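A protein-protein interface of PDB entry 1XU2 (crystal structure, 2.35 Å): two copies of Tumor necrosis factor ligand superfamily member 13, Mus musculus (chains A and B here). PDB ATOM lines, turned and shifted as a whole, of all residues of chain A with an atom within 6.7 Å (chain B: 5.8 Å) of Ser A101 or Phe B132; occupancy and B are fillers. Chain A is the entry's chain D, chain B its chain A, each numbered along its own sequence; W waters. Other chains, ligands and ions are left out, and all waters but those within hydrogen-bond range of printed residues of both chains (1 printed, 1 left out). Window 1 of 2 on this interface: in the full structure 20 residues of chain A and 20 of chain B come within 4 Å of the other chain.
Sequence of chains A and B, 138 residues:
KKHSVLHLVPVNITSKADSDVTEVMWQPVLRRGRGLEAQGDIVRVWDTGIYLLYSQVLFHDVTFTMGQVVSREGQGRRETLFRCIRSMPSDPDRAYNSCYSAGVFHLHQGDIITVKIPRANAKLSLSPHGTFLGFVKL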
ATOM      1  N   LEU A  53      11.354 -11.951  21.127  1.00  0.00           N
ATOM      2  CA  LEU A  53      12.121 -13.018  21.764  1.00  0.00           C
ATOM      3  C   LEU A  53      11.250 -13.596  22.885  1.00  0.00           C
ATOM      4  O   LEU A  53      10.764 -12.854  23.732  1.00  0.00           O
ATOM      5  CB  LEU A  53      13.376 -12.398  22.360  1.00  0.00           C
ATOM      6  CG  LEU A  53      14.646 -13.211  22.513  1.00  0.00           C
ATOM      7  CD1 LEU A  53      15.764 -12.289  22.949  1.00  0.00           C
ATOM      8  CD2 LEU A  53      14.452 -14.328  23.515  1.00  0.00           C
ATOM      9  N   TYR A  54      11.032 -14.906  22.882  1.00  0.00           N
ATOM     10  CA  TYR A  54      10.268 -15.551  23.943  1.00  0.00           C
ATOM     11  C   TYR A  54      11.041 -16.743  24.536  1.00  0.00           C
ATOM     12  O   TYR A  54      11.834 -17.383  23.863  1.00  0.00           O
ATOM     13  CB  TYR A  54       8.868 -15.955  23.444  1.00  0.00           C
ATOM     14  CG  TYR A  54       8.857 -16.957  22.322  1.00  0.00           C
ATOM     15  CD1 TYR A  54       8.897 -18.329  22.585  1.00  0.00           C
ATOM     16  CD2 TYR A  54       8.798 -16.541  20.997  1.00  0.00           C
ATOM     17  CE1 TYR A  54       8.887 -19.260  21.549  1.00  0.00           C
ATOM     18  CE2 TYR A  54       8.786 -17.455  19.962  1.00  0.00           C
ATOM     19  CZ  TYR A  54       8.836 -18.818  20.243  1.00  0.00           C
ATOM     20  OH  TYR A  54       8.823 -19.727  19.208  1.00  0.00           O
ATOM     21  N   SER A  55      10.778 -17.028  25.804  1.00  0.00           N
ATOM     22  CA  SER A  55      11.525 -18.011  26.566  1.00  0.00           C
ATOM     23  C   SER A  55      10.625 -18.646  27.594  1.00  0.00           C
ATOM     24  O   SER A  55      10.019 -17.946  28.384  1.00  0.00           O
ATOM     25  CB  SER A  55      12.691 -17.345  27.293  1.00  0.00           C
ATOM     26  OG  SER A  55      13.365 -18.241  28.169  1.00  0.00           O
ATOM     27  N   GLN A  56      10.532 -19.974  27.578  1.00  0.00           N
ATOM     28  CA  GLN A  56       9.887 -20.699  28.664  1.00  0.00           C
ATOM     29  C   GLN A  56      10.835 -21.752  29.228  1.00  0.00           C
ATOM     30  O   GLN A  56      11.580 -22.401  28.490  1.00  0.00           O
ATOM     31  CB  GLN A  56       8.582 -21.362  28.210  1.00  0.00           C
ATOM     32  CG  GLN A  56       7.924 -22.237  29.307  1.00  0.00           C
ATOM     33  CD  GLN A  56       6.506 -22.632  28.977  1.00  0.00           C
ATOM     34  OE1 GLN A  56       5.662 -21.770  28.783  1.00  0.00           O
ATOM     35  NE2 GLN A  56       6.242 -23.936  28.912  1.00  0.00           N
ATOM     36  N   VAL A  57      10.805 -21.908  30.545  1.00  0.00           N
ATOM     37  CA  VAL A  57      11.489 -23.012  31.211  1.00  0.00           C
ATOM     38  C   VAL A  57      10.530 -23.687  32.175  1.00  0.00           C
ATOM     39  O   VAL A  57       9.779 -23.019  32.868  1.00  0.00           O
ATOM     40  CB  VAL A  57      12.732 -22.556  31.982  1.00  0.00           C
ATOM     41  CG1 VAL A  57      13.438 -23.773  32.591  1.00  0.00           C
ATOM     42  CG2 VAL A  57      13.673 -21.771  31.068  1.00  0.00           C
ATOM     43  N   GLN A  68      14.575 -17.691  34.910  1.00  0.00           N
ATOM     44  CA  GLN A  68      15.615 -17.550  33.906  1.00  0.00           C
ATOM     45  C   GLN A  68      15.883 -16.092  33.548  1.00  0.00           C
ATOM     46  O   GLN A  68      15.013 -15.253  33.617  1.00  0.00           O
ATOM     47  CB  GLN A  68      15.287 -18.387  32.650  1.00  0.00           C
ATOM     48  CG  GLN A  68      14.186 -17.825  31.728  1.00  0.00           C
ATOM     49  CD  GLN A  68      12.806 -18.399  32.027  1.00  0.00           C
ATOM     50  OE1 GLN A  68      12.559 -18.906  33.131  1.00  0.00           O
ATOM     51  NE2 GLN A  68      11.897 -18.308  31.050  1.00  0.00           N
ATOM     52  N   VAL A  70      17.409 -13.843  30.483  1.00  0.00           N
ATOM     53  CA  VAL A  70      17.760 -13.795  29.067  1.00  0.00           C
ATOM     54  C   VAL A  70      18.533 -12.511  28.826  1.00  0.00           C
ATOM     55  O   VAL A  70      18.081 -11.436  29.197  1.00  0.00           O
ATOM     56  CB  VAL A  70      16.495 -13.844  28.193  1.00  0.00           C
ATOM     57  CG1 VAL A  70      16.842 -13.819  26.700  1.00  0.00           C
ATOM     58  CG2 VAL A  70      15.703 -15.083  28.531  1.00  0.00           C
ATOM     59  N   LEU A  81      17.830  -8.647  29.213  1.00  0.00           N
ATOM     60  CA  LEU A  81      16.691  -8.266  28.394  1.00  0.00           C
ATOM     61  C   LEU A  81      15.409  -8.469  29.188  1.00  0.00           C
ATOM     62  O   LEU A  81      14.596  -7.552  29.325  1.00  0.00           O
ATOM     63  CB  LEU A  81      16.659  -9.088  27.103  1.00  0.00           C
ATOM     64  CG  LEU A  81      17.837  -8.906  26.131  1.00  0.00           C
ATOM     65  CD1 LEU A  81      17.605  -9.749  24.888  1.00  0.00           C
ATOM     66  CD2 LEU A  81      18.075  -7.440  25.742  1.00  0.00           C
ATOM     67  N   PHE A  82      15.232  -9.673  29.712  1.00  0.00           N
ATOM     68  CA  PHE A  82      14.119  -9.954  30.619  1.00  0.00           C
ATOM     69  C   PHE A  82      14.385 -11.130  31.553  1.00  0.00           C
ATOM     70  O   PHE A  82      15.210 -11.996  31.274  1.00  0.00           O
ATOM     71  CB  PHE A  82      12.783 -10.140  29.867  1.00  0.00           C
ATOM     72  CG  PHE A  82      12.776 -11.259  28.865  1.00  0.00           C
ATOM     73  CD1 PHE A  82      12.427 -12.541  29.239  1.00  0.00           C
ATOM     74  CD2 PHE A  82      13.071 -11.016  27.540  1.00  0.00           C
ATOM     75  CE1 PHE A  82      12.407 -13.559  28.319  1.00  0.00           C
ATOM     76  CE2 PHE A  82      13.051 -12.031  26.616  1.00  0.00           C
ATOM     77  CZ  PHE A  82      12.712 -13.301  27.001  1.00  0.00           C
ATOM     78  N   ARG A  83      13.696 -11.102  32.685  1.00  0.00           N
ATOM     79  CA  ARG A  83      13.719 -12.150  33.687  1.00  0.00           C
ATOM     80  C   ARG A  83      12.307 -12.708  33.891  1.00  0.00           C
ATOM     81  O   ARG A  83      11.314 -11.981  33.788  1.00  0.00           O
ATOM     82  CB  ARG A  83      14.174 -11.584  35.024  1.00  0.00           C
ATOM     83  CG  ARG A  83      15.631 -11.272  35.131  1.00  0.00           C
ATOM     84  CD  ARG A  83      15.896  -9.995  35.935  1.00  0.00           C
ATOM     85  NE  ARG A  83      15.493 -10.154  37.316  1.00  0.00           N
ATOM     86  CZ  ARG A  83      15.064  -9.186  38.122  1.00  0.00           C
ATOM     87  NH1 ARG A  83      14.933  -7.922  37.722  1.00  0.00           N
ATOM     88  NH2 ARG A  83      14.763  -9.501  39.367  1.00  0.00           N
ATOM     89  N   CYS A  84      12.235 -13.992  34.197  1.00  0.00           N
ATOM     90  CA  CYS A  84      11.005 -14.633  34.656  1.00  0.00           C
ATOM     91  C   CYS A  84      11.306 -15.214  36.052  1.00  0.00           C
ATOM     92  O   CYS A  84      12.395 -15.742  36.275  1.00  0.00           O
ATOM     93  CB  CYS A  84      10.565 -15.715  33.657  1.00  0.00           C
ATOM     94  SG  CYS A  84       8.972 -16.488  34.032  1.00  0.00           S
ATOM     95  N   CYS A  99       7.749 -21.179  33.578  1.00  0.00           N
ATOM     96  CA  CYS A  99       8.035 -19.760  33.686  1.00  0.00           C
ATOM     97  C   CYS A  99       8.234 -19.230  32.254  1.00  0.00           C
ATOM     98  O   CYS A  99       9.187 -19.602  31.574  1.00  0.00           O
ATOM     99  CB  CYS A  99       9.286 -19.553  34.541  1.00  0.00           C
ATOM    100  SG  CYS A  99       9.315 -17.977  35.398  1.00  0.00           S
ATOM    101  N   TYR A 100       7.310 -18.396  31.804  1.00  0.00           N
ATOM    102  CA  TYR A 100       7.315 -17.855  30.449  1.00  0.00           C
ATOM    103  C   TYR A 100       7.458 -16.348  30.518  1.00  0.00           C
ATOM    104  O   TYR A 100       6.830 -15.689  31.359  1.00  0.00           O
ATOM    105  CB  TYR A 100       6.019 -18.208  29.691  1.00  0.00           C
ATOM    106  CG  TYR A 100       5.948 -17.628  28.281  1.00  0.00           C
ATOM    107  CD1 TYR A 100       5.611 -16.291  28.065  1.00  0.00           C
ATOM    108  CD2 TYR A 100       6.215 -18.418  27.156  1.00  0.00           C
ATOM    109  CE1 TYR A 100       5.562 -15.756  26.778  1.00  0.00           C
ATOM    110  CE2 TYR A 100       6.160 -17.882  25.860  1.00  0.00           C
ATOM    111  CZ  TYR A 100       5.838 -16.558  25.683  1.00  0.00           C
ATOM    112  OH  TYR A 100       5.766 -16.015  24.423  1.00  0.00           O
ATOM    113  N   SER A 101       8.292 -15.809  29.633  1.00  0.00           N
ATOM    114  CA  SER A 101       8.362 -14.377  29.417  1.00  0.00           C
ATOM    115  C   SER A 101       8.836 -14.078  28.010  1.00  0.00           C
ATOM    116  O   SER A 101       9.386 -14.946  27.326  1.00  0.00           O
ATOM    117  CB  SER A 101       9.294 -13.713  30.429  1.00  0.00           C
ATOM    118  OG  SER A 101       9.210 -12.301  30.315  1.00  0.00           O
ATOM    119  N   ALA A 102       8.608 -12.838  27.582  1.00  0.00           N
ATOM    120  CA  ALA A 102       8.924 -12.419  26.223  1.00  0.00           C
ATOM    121  C   ALA A 102       8.945 -10.906  26.090  1.00  0.00           C
ATOM    122  O   ALA A 102       8.343 -10.176  26.883  1.00  0.00           O
ATOM    123  CB  ALA A 102       7.914 -12.996  25.252  1.00  0.00           C
ATOM    124  N   GLY A 103       9.635 -10.435  25.065  1.00  0.00           N
ATOM    125  CA  GLY A 103       9.616  -9.023  24.729  1.00  0.00           C
ATOM    126  C   GLY A 103      10.205  -8.777  23.364  1.00  0.00           C
ATOM    127  O   GLY A 103      10.647  -9.701  22.704  1.00  0.00           O
ATOM    128  N   VAL A 104      10.224  -7.512  22.971  1.00  0.00           N
ATOM    129  CA  VAL A 104      10.770  -7.075  21.708  1.00  0.00           C
ATOM    130  C   VAL A 104      12.052  -6.271  21.947  1.00  0.00           C
ATOM    131  O   VAL A 104      12.073  -5.323  22.732  1.00  0.00           O
ATOM    132  CB  VAL A 104       9.736  -6.209  20.974  1.00  0.00           C
ATOM    133  CG1 VAL A 104      10.292  -5.715  19.666  1.00  0.00           C
ATOM    134  CG2 VAL A 104       8.453  -7.009  20.757  1.00  0.00           C
ATOM    135  N   PHE A 105      13.118  -6.642  21.247  1.00  0.00           N
ATOM    136  CA  PHE A 105      14.431  -6.058  21.478  1.00  0.00           C
ATOM    137  C   PHE A 105      15.177  -5.819  20.176  1.00  0.00           C
ATOM    138  O   PHE A 105      15.036  -6.568  19.224  1.00  0.00           O
ATOM    139  CB  PHE A 105      15.240  -6.967  22.409  1.00  0.00           C
ATOM    140  CG  PHE A 105      14.552  -7.219  23.710  1.00  0.00           C
ATOM    141  CD1 PHE A 105      14.637  -6.291  24.732  1.00  0.00           C
ATOM    142  CD2 PHE A 105      13.760  -8.334  23.883  1.00  0.00           C
ATOM    143  CE1 PHE A 105      13.962  -6.481  25.917  1.00  0.00           C
ATOM    144  CE2 PHE A 105      13.072  -8.535  25.063  1.00  0.00           C
ATOM    145  CZ  PHE A 105      13.181  -7.614  26.084  1.00  0.00           C
ATOM    146  N   HIS B   7       8.430  -0.659  23.196  1.00  0.00           N
ATOM    147  CA  HIS B   7       8.730  -1.387  24.411  1.00  0.00           C
ATOM    148  C   HIS B   7       8.969  -0.365  25.519  1.00  0.00           C
ATOM    149  O   HIS B   7       9.807   0.513  25.373  1.00  0.00           O
ATOM    150  CB  HIS B   7       9.945  -2.301  24.206  1.00  0.00           C
ATOM    151  CG  HIS B   7      10.202  -3.238  25.344  1.00  0.00           C
ATOM    152  ND1 HIS B   7       9.430  -4.357  25.577  1.00  0.00           N
ATOM    153  CD2 HIS B   7      11.153  -3.226  26.311  1.00  0.00           C
ATOM    154  CE1 HIS B   7       9.899  -4.994  26.640  1.00  0.00           C
ATOM    155  NE2 HIS B   7      10.938  -4.321  27.107  1.00  0.00           N
ATOM    156  N   LEU B   8       8.215  -0.497  26.613  1.00  0.00           N
ATOM    157  CA  LEU B   8       8.198   0.452  27.736  1.00  0.00           C
ATOM    158  C   LEU B   8       8.652  -0.175  29.058  1.00  0.00           C
ATOM    159  O   LEU B   8       8.296  -1.317  29.359  1.00  0.00           O
ATOM    160  CB  LEU B   8       6.792   0.981  27.949  1.00  0.00           C
ATOM    161  CG  LEU B   8       6.128   1.589  26.709  1.00  0.00           C
ATOM    162  CD1 LEU B   8       4.625   1.583  26.860  1.00  0.00           C
ATOM    163  CD2 LEU B   8       6.633   2.987  26.474  1.00  0.00           C
ATOM    164  N   VAL B   9       9.387   0.606  29.853  1.00  0.00           N
ATOM    165  CA  VAL B   9       9.802   0.227  31.202  1.00  0.00           C
ATOM    166  C   VAL B   9       9.412   1.307  32.233  1.00  0.00           C
ATOM    167  O   VAL B   9       9.132   2.451  31.860  1.00  0.00           O
ATOM    168  CB  VAL B   9      11.317  -0.039  31.265  1.00  0.00           C
ATOM    169  CG1 VAL B   9      11.709  -1.124  30.262  1.00  0.00           C
ATOM    170  CG2 VAL B   9      12.130   1.243  31.038  1.00  0.00           C
ATOM    171  N   PRO B  10       9.386   0.955  33.523  1.00  0.00           N
ATOM    172  CA  PRO B  10       8.997   1.906  34.566  1.00  0.00           C
ATOM    173  C   PRO B  10       9.967   3.055  34.764  1.00  0.00           C
ATOM    174  O   PRO B  10      11.193   2.895  34.630  1.00  0.00           O
ATOM    175  CB  PRO B  10       8.994   1.048  35.842  1.00  0.00           C
ATOM    176  CG  PRO B  10       8.950  -0.334  35.388  1.00  0.00           C
ATOM    177  CD  PRO B  10       9.686  -0.366  34.099  1.00  0.00           C
ATOM    178  N   TRP B  26       5.345   5.035  32.660  1.00  0.00           N
ATOM    179  CA  TRP B  26       6.127   4.321  31.633  1.00  0.00           C
ATOM    180  C   TRP B  26       7.049   5.245  30.846  1.00  0.00           C
ATOM    181  O   TRP B  26       6.733   6.416  30.631  1.00  0.00           O
ATOM    182  CB  TRP B  26       5.191   3.617  30.635  1.00  0.00           C
ATOM    183  CG  TRP B  26       4.313   2.593  31.249  1.00  0.00           C
ATOM    184  CD1 TRP B  26       2.972   2.696  31.483  1.00  0.00           C
ATOM    185  CD2 TRP B  26       4.710   1.307  31.737  1.00  0.00           C
ATOM    186  NE1 TRP B  26       2.507   1.551  32.082  1.00  0.00           N
ATOM    187  CE2 TRP B  26       3.554   0.681  32.253  1.00  0.00           C
ATOM    188  CE3 TRP B  26       5.928   0.620  31.792  1.00  0.00           C
ATOM    189  CZ2 TRP B  26       3.579  -0.596  32.817  1.00  0.00           C
ATOM    190  CZ3 TRP B  26       5.960  -0.641  32.345  1.00  0.00           C
ATOM    191  CH2 TRP B  26       4.787  -1.245  32.857  1.00  0.00           C
ATOM    192  N   TYR B  54       1.654  -6.900  25.228  1.00  0.00           N
ATOM    193  CA  TYR B  54       2.195  -7.755  26.275  1.00  0.00           C
ATOM    194  C   TYR B  54       2.590  -6.952  27.502  1.00  0.00           C
ATOM    195  O   TYR B  54       3.011  -5.805  27.398  1.00  0.00           O
ATOM    196  CB  TYR B  54       3.374  -8.591  25.754  1.00  0.00           C
ATOM    197  CG  TYR B  54       4.549  -7.797  25.257  1.00  0.00           C
ATOM    198  CD1 TYR B  54       5.558  -7.398  26.126  1.00  0.00           C
ATOM    199  CD2 TYR B  54       4.665  -7.455  23.916  1.00  0.00           C
ATOM    200  CE1 TYR B  54       6.656  -6.672  25.673  1.00  0.00           C
ATOM    201  CE2 TYR B  54       5.753  -6.727  23.460  1.00  0.00           C
ATOM    202  CZ  TYR B  54       6.749  -6.338  24.343  1.00  0.00           C
ATOM    203  OH  TYR B  54       7.841  -5.610  23.898  1.00  0.00           O
ATOM    204  N   SER B  55       2.447  -7.592  28.661  1.00  0.00           N
ATOM    205  CA  SER B  55       2.630  -6.962  29.965  1.00  0.00           C
ATOM    206  C   SER B  55       3.238  -7.963  30.934  1.00  0.00           C
ATOM    207  O   SER B  55       2.771  -9.090  31.049  1.00  0.00           O
ATOM    208  CB  SER B  55       1.292  -6.474  30.529  1.00  0.00           C
ATOM    209  OG  SER B  55       1.401  -6.063  31.893  1.00  0.00           O
ATOM    210  N   GLN B  56       4.318  -7.549  31.576  1.00  0.00           N
ATOM    211  CA  GLN B  56       4.872  -8.261  32.695  1.00  0.00           C
ATOM    212  C   GLN B  56       5.016  -7.337  33.882  1.00  0.00           C
ATOM    213  O   GLN B  56       5.477  -6.208  33.740  1.00  0.00           O
ATOM    214  CB  GLN B  56       6.256  -8.838  32.376  1.00  0.00           C
ATOM    215  CG  GLN B  56       6.816  -9.623  33.567  1.00  0.00           C
ATOM    216  CD  GLN B  56       7.968 -10.510  33.197  1.00  0.00           C
ATOM    217  OE1 GLN B  56       7.805 -11.448  32.409  1.00  0.00           O
ATOM    218  NE2 GLN B  56       9.139 -10.234  33.771  1.00  0.00           N
ATOM    219  N   VAL B  57       4.661  -7.842  35.057  1.00  0.00           N
ATOM    220  CA  VAL B  57       4.993  -7.172  36.306  1.00  0.00           C
ATOM    221  C   VAL B  57       5.673  -8.148  37.246  1.00  0.00           C
ATOM    222  O   VAL B  57       5.242  -9.301  37.396  1.00  0.00           O
ATOM    223  CB  VAL B  57       3.745  -6.593  36.983  1.00  0.00           C
ATOM    224  CG1 VAL B  57       4.139  -5.754  38.194  1.00  0.00           C
ATOM    225  CG2 VAL B  57       2.924  -5.756  35.983  1.00  0.00           C
ATOM    226  N   TYR B 100       3.191 -12.548  33.587  1.00  0.00           N
ATOM    227  CA  TYR B 100       3.255 -12.210  32.178  1.00  0.00           C
ATOM    228  C   TYR B 100       1.963 -12.621  31.505  1.00  0.00           C
ATOM    229  O   TYR B 100       1.487 -13.755  31.666  1.00  0.00           O
ATOM    230  CB  TYR B 100       4.440 -12.910  31.481  1.00  0.00           C
ATOM    231  CG  TYR B 100       4.529 -12.570  30.001  1.00  0.00           C
ATOM    232  CD1 TYR B 100       3.711 -13.205  29.071  1.00  0.00           C
ATOM    233  CD2 TYR B 100       5.396 -11.575  29.539  1.00  0.00           C
ATOM    234  CE1 TYR B 100       3.765 -12.867  27.718  1.00  0.00           C
ATOM    235  CE2 TYR B 100       5.454 -11.236  28.184  1.00  0.00           C
ATOM    236  CZ  TYR B 100       4.628 -11.881  27.289  1.00  0.00           C
ATOM    237  OH  TYR B 100       4.670 -11.582  25.951  1.00  0.00           O
ATOM    238  N   SER B 127      12.587  -2.534  37.907  1.00  0.00           N
ATOM    239  CA  SER B 127      13.622  -3.046  37.022  1.00  0.00           C
ATOM    240  C   SER B 127      13.073  -3.147  35.603  1.00  0.00           C
ATOM    241  O   SER B 127      11.968  -3.635  35.411  1.00  0.00           O
ATOM    242  CB  SER B 127      14.084  -4.421  37.482  1.00  0.00           C
ATOM    243  OG  SER B 127      14.987  -4.976  36.551  1.00  0.00           O
ATOM    244  N   PRO B 128      13.826  -2.666  34.617  1.00  0.00           N
ATOM    245  CA  PRO B 128      13.348  -2.678  33.233  1.00  0.00           C
ATOM    246  C   PRO B 128      13.207  -4.092  32.669  1.00  0.00           C
ATOM    247  O   PRO B 128      12.408  -4.299  31.744  1.00  0.00           O
ATOM    248  CB  PRO B 128      14.409  -1.861  32.480  1.00  0.00           C
ATOM    249  CG  PRO B 128      15.629  -1.885  33.340  1.00  0.00           C
ATOM    250  CD  PRO B 128      15.166  -2.060  34.742  1.00  0.00           C
ATOM    251  N   HIS B 129      13.935  -5.048  33.245  1.00  0.00           N
ATOM    252  CA  HIS B 129      13.854  -6.438  32.816  1.00  0.00           C
ATOM    253  C   HIS B 129      12.906  -7.296  33.685  1.00  0.00           C
ATOM    254  O   HIS B 129      12.683  -8.459  33.367  1.00  0.00           O
ATOM    255  CB  HIS B 129      15.251  -7.104  32.650  1.00  0.00           C
ATOM    256  CG  HIS B 129      16.292  -6.656  33.630  1.00  0.00           C
ATOM    257  ND1 HIS B 129      16.218  -6.929  34.979  1.00  0.00           N
ATOM    258  CD2 HIS B 129      17.467  -6.005  33.446  1.00  0.00           C
ATOM    259  CE1 HIS B 129      17.287  -6.442  35.586  1.00  0.00           C
ATOM    260  NE2 HIS B 129      18.062  -5.882  34.677  1.00  0.00           N
ATOM    261  N   GLY B 130      12.321  -6.722  34.738  1.00  0.00           N
ATOM    262  CA  GLY B 130      11.323  -7.418  35.546  1.00  0.00           C
ATOM    263  C   GLY B 130       9.884  -6.995  35.277  1.00  0.00           C
ATOM    264  O   GLY B 130       8.949  -7.815  35.326  1.00  0.00           O
ATOM    265  N   THR B 131       9.718  -5.704  35.000  1.00  0.00           N
ATOM    266  CA  THR B 131       8.433  -5.091  34.741  1.00  0.00           C
ATOM    267  C   THR B 131       8.531  -4.284  33.452  1.00  0.00           C
ATOM    268  O   THR B 131       9.423  -3.447  33.305  1.00  0.00           O
ATOM    269  CB  THR B 131       8.056  -4.168  35.912  1.00  0.00           C
ATOM    270  OG1 THR B 131       7.897  -4.931  37.124  1.00  0.00           O
ATOM    271  CG2 THR B 131       6.692  -3.515  35.677  1.00  0.00           C
ATOM    272  N   PHE B 132       7.616  -4.535  32.516  1.00  0.00           N
ATOM    273  CA  PHE B 132       7.635  -3.862  31.224  1.00  0.00           C
ATOM    274  C   PHE B 132       6.295  -4.046  30.500  1.00  0.00           C
ATOM    275  O   PHE B 132       5.430  -4.798  30.943  1.00  0.00           O
ATOM    276  CB  PHE B 132       8.817  -4.343  30.354  1.00  0.00           C
ATOM    277  CG  PHE B 132       8.919  -5.844  30.244  1.00  0.00           C
ATOM    278  CD1 PHE B 132       8.064  -6.554  29.398  1.00  0.00           C
ATOM    279  CD2 PHE B 132       9.836  -6.547  31.013  1.00  0.00           C
ATOM    280  CE1 PHE B 132       8.143  -7.925  29.303  1.00  0.00           C
ATOM    281  CE2 PHE B 132       9.923  -7.935  30.931  1.00  0.00           C
ATOM    282  CZ  PHE B 132       9.084  -8.631  30.077  1.00  0.00           C
ATOM    283  N   LEU B 133       6.142  -3.334  29.393  1.00  0.00           N
ATOM    284  CA  LEU B 133       4.893  -3.273  28.655  1.00  0.00           C
ATOM    285  C   LEU B 133       5.207  -2.949  27.189  1.00  0.00           C
ATOM    286  O   LEU B 133       6.004  -2.062  26.902  1.00  0.00           O
ATOM    287  CB  LEU B 133       4.008  -2.207  29.279  1.00  0.00           C
ATOM    288  CG  LEU B 133       2.798  -1.717  28.475  1.00  0.00           C
ATOM    289  CD1 LEU B 133       1.716  -2.774  28.450  1.00  0.00           C
ATOM    290  CD2 LEU B 133       2.270  -0.420  29.063  1.00  0.00           C
ATOM    291  N   GLY B 134       4.597  -3.671  26.258  1.00  0.00           N
ATOM    292  CA  GLY B 134       4.928  -3.494  24.857  1.00  0.00           C
ATOM    293  C   GLY B 134       3.830  -3.776  23.856  1.00  0.00           C
ATOM    294  O   GLY B 134       2.793  -4.374  24.191  1.00  0.00           O
HETATM  295  O   HOH W   1       3.862 -13.818  24.258  1.00  0.00           O
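N of Val A104 sits at hydrogen-bond distance from OH of Tyr B54.
The side-chain amide nitrogen (NE2) of Gln B56 lies within hydrogen-bond range of the backbone carbonyl oxygen (O) of Arg A83 (2.8 Å).
The side-chain hydroxyl of Ser A101 lies within hydrogen-bond range of the side-chain amide oxygen of Gln B56 (2.7 Å).
NH1 of Arg A83 is in hydrogen-bond range of OG of Ser B127 (3.2 Å).
The backbone carbonyl oxygen (O) of His B129 is in hydrogen-bond range of the backbone NH (N) of Arg A83, at 2.9 Å.
N of Gly B134 lies within hydrogen-bond range of O of Tyr B54 (2.9 Å).
The backbone NH (N) of Leu A53 is in hydrogen-bond range of the backbone carbonyl oxygen (O) of Gly A103 (2.8 Å).
N of Ser A55 lies within hydrogen-bond range of O of Ser A101.
N of Val A70 sits at hydrogen-bond distance from O of Phe A82 (3.0 Å).
The backbone NH (N) of Tyr A100 is in hydrogen-bond range of the side-chain sulfur (SG) of Cys A84 (3.4 Å).
SG of Cys A84 forms a disulfide with SG of Cys A99.
Among the printed residues, pairs that only touch across the chains: Ala A102 with Phe B132 (3.3 Å), Ala A102 with Tyr B100 (3.3 Å), Leu A81 with His B129 (3.4 Å), Phe A82 with His B129 (3.4 Å), Tyr A100 with Tyr B100 (3.5 Å), Ser A101 with Phe B132 (3.7 Å), Phe A82 with Phe B132 (3.8 Å), Val A104 with His B7 (3.8 Å), Gly A103 with Tyr B54 (3.9 Å), Phe A105 with His B7 (3.9 Å) and Ser A101 with Tyr B100 (3.96 Å).
Ser A101 touches three residues of chain B.
Of the printed residues of chain B, Arg A83 touches Gln B56 (2.8 Å), Ser B127 (3.2 Å) and His B129 (2.9 Å).
Of the printed residues of chain A, His B7 touches Val A104 and Phe A105.
Printed residues of chain B within 4 Å of Leu A81: His B129.
Of the printed residues of chain B, Phe A105 touches His B7.
Cys A84 touches none of the printed residues of chain B.
Cys A99 touches none of the printed residues of chain B.
The nearest printed residue of chain B that does not touch Ser A101 is His B129 (6.0 Å).
The nearest printed residue of chain A that does not touch Phe B132 is Gly A103 (4.9 Å).
The nearest printed residue of chain B that does not touch Gly A103 is His B7 (4.5 Å).
Printed residues of chain B that touch a printed residue of chain A: His B7, Tyr B54, Gln B56, Tyr B100, Ser B127, His B129 and Phe B132.
Hydrophobic or aromatic side chains of chain B within 4 Å of the printed part of chain A: His B7, Tyr B54, Tyr B100, His B129 and Phe B132.
Tyr A100 touches its own counterpart, Tyr B100.
5 positions are printed for both chains.
Of the 16 pairs that touch across the chains among the printed residues, 1 has its exchanged pair printed and touching as well.
Water W1 bridges the side-chain hydroxyl (OH) of Tyr A100 (2.9 Å) and the side-chain hydroxyl (OH) of Tyr B100 (2.9 Å).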
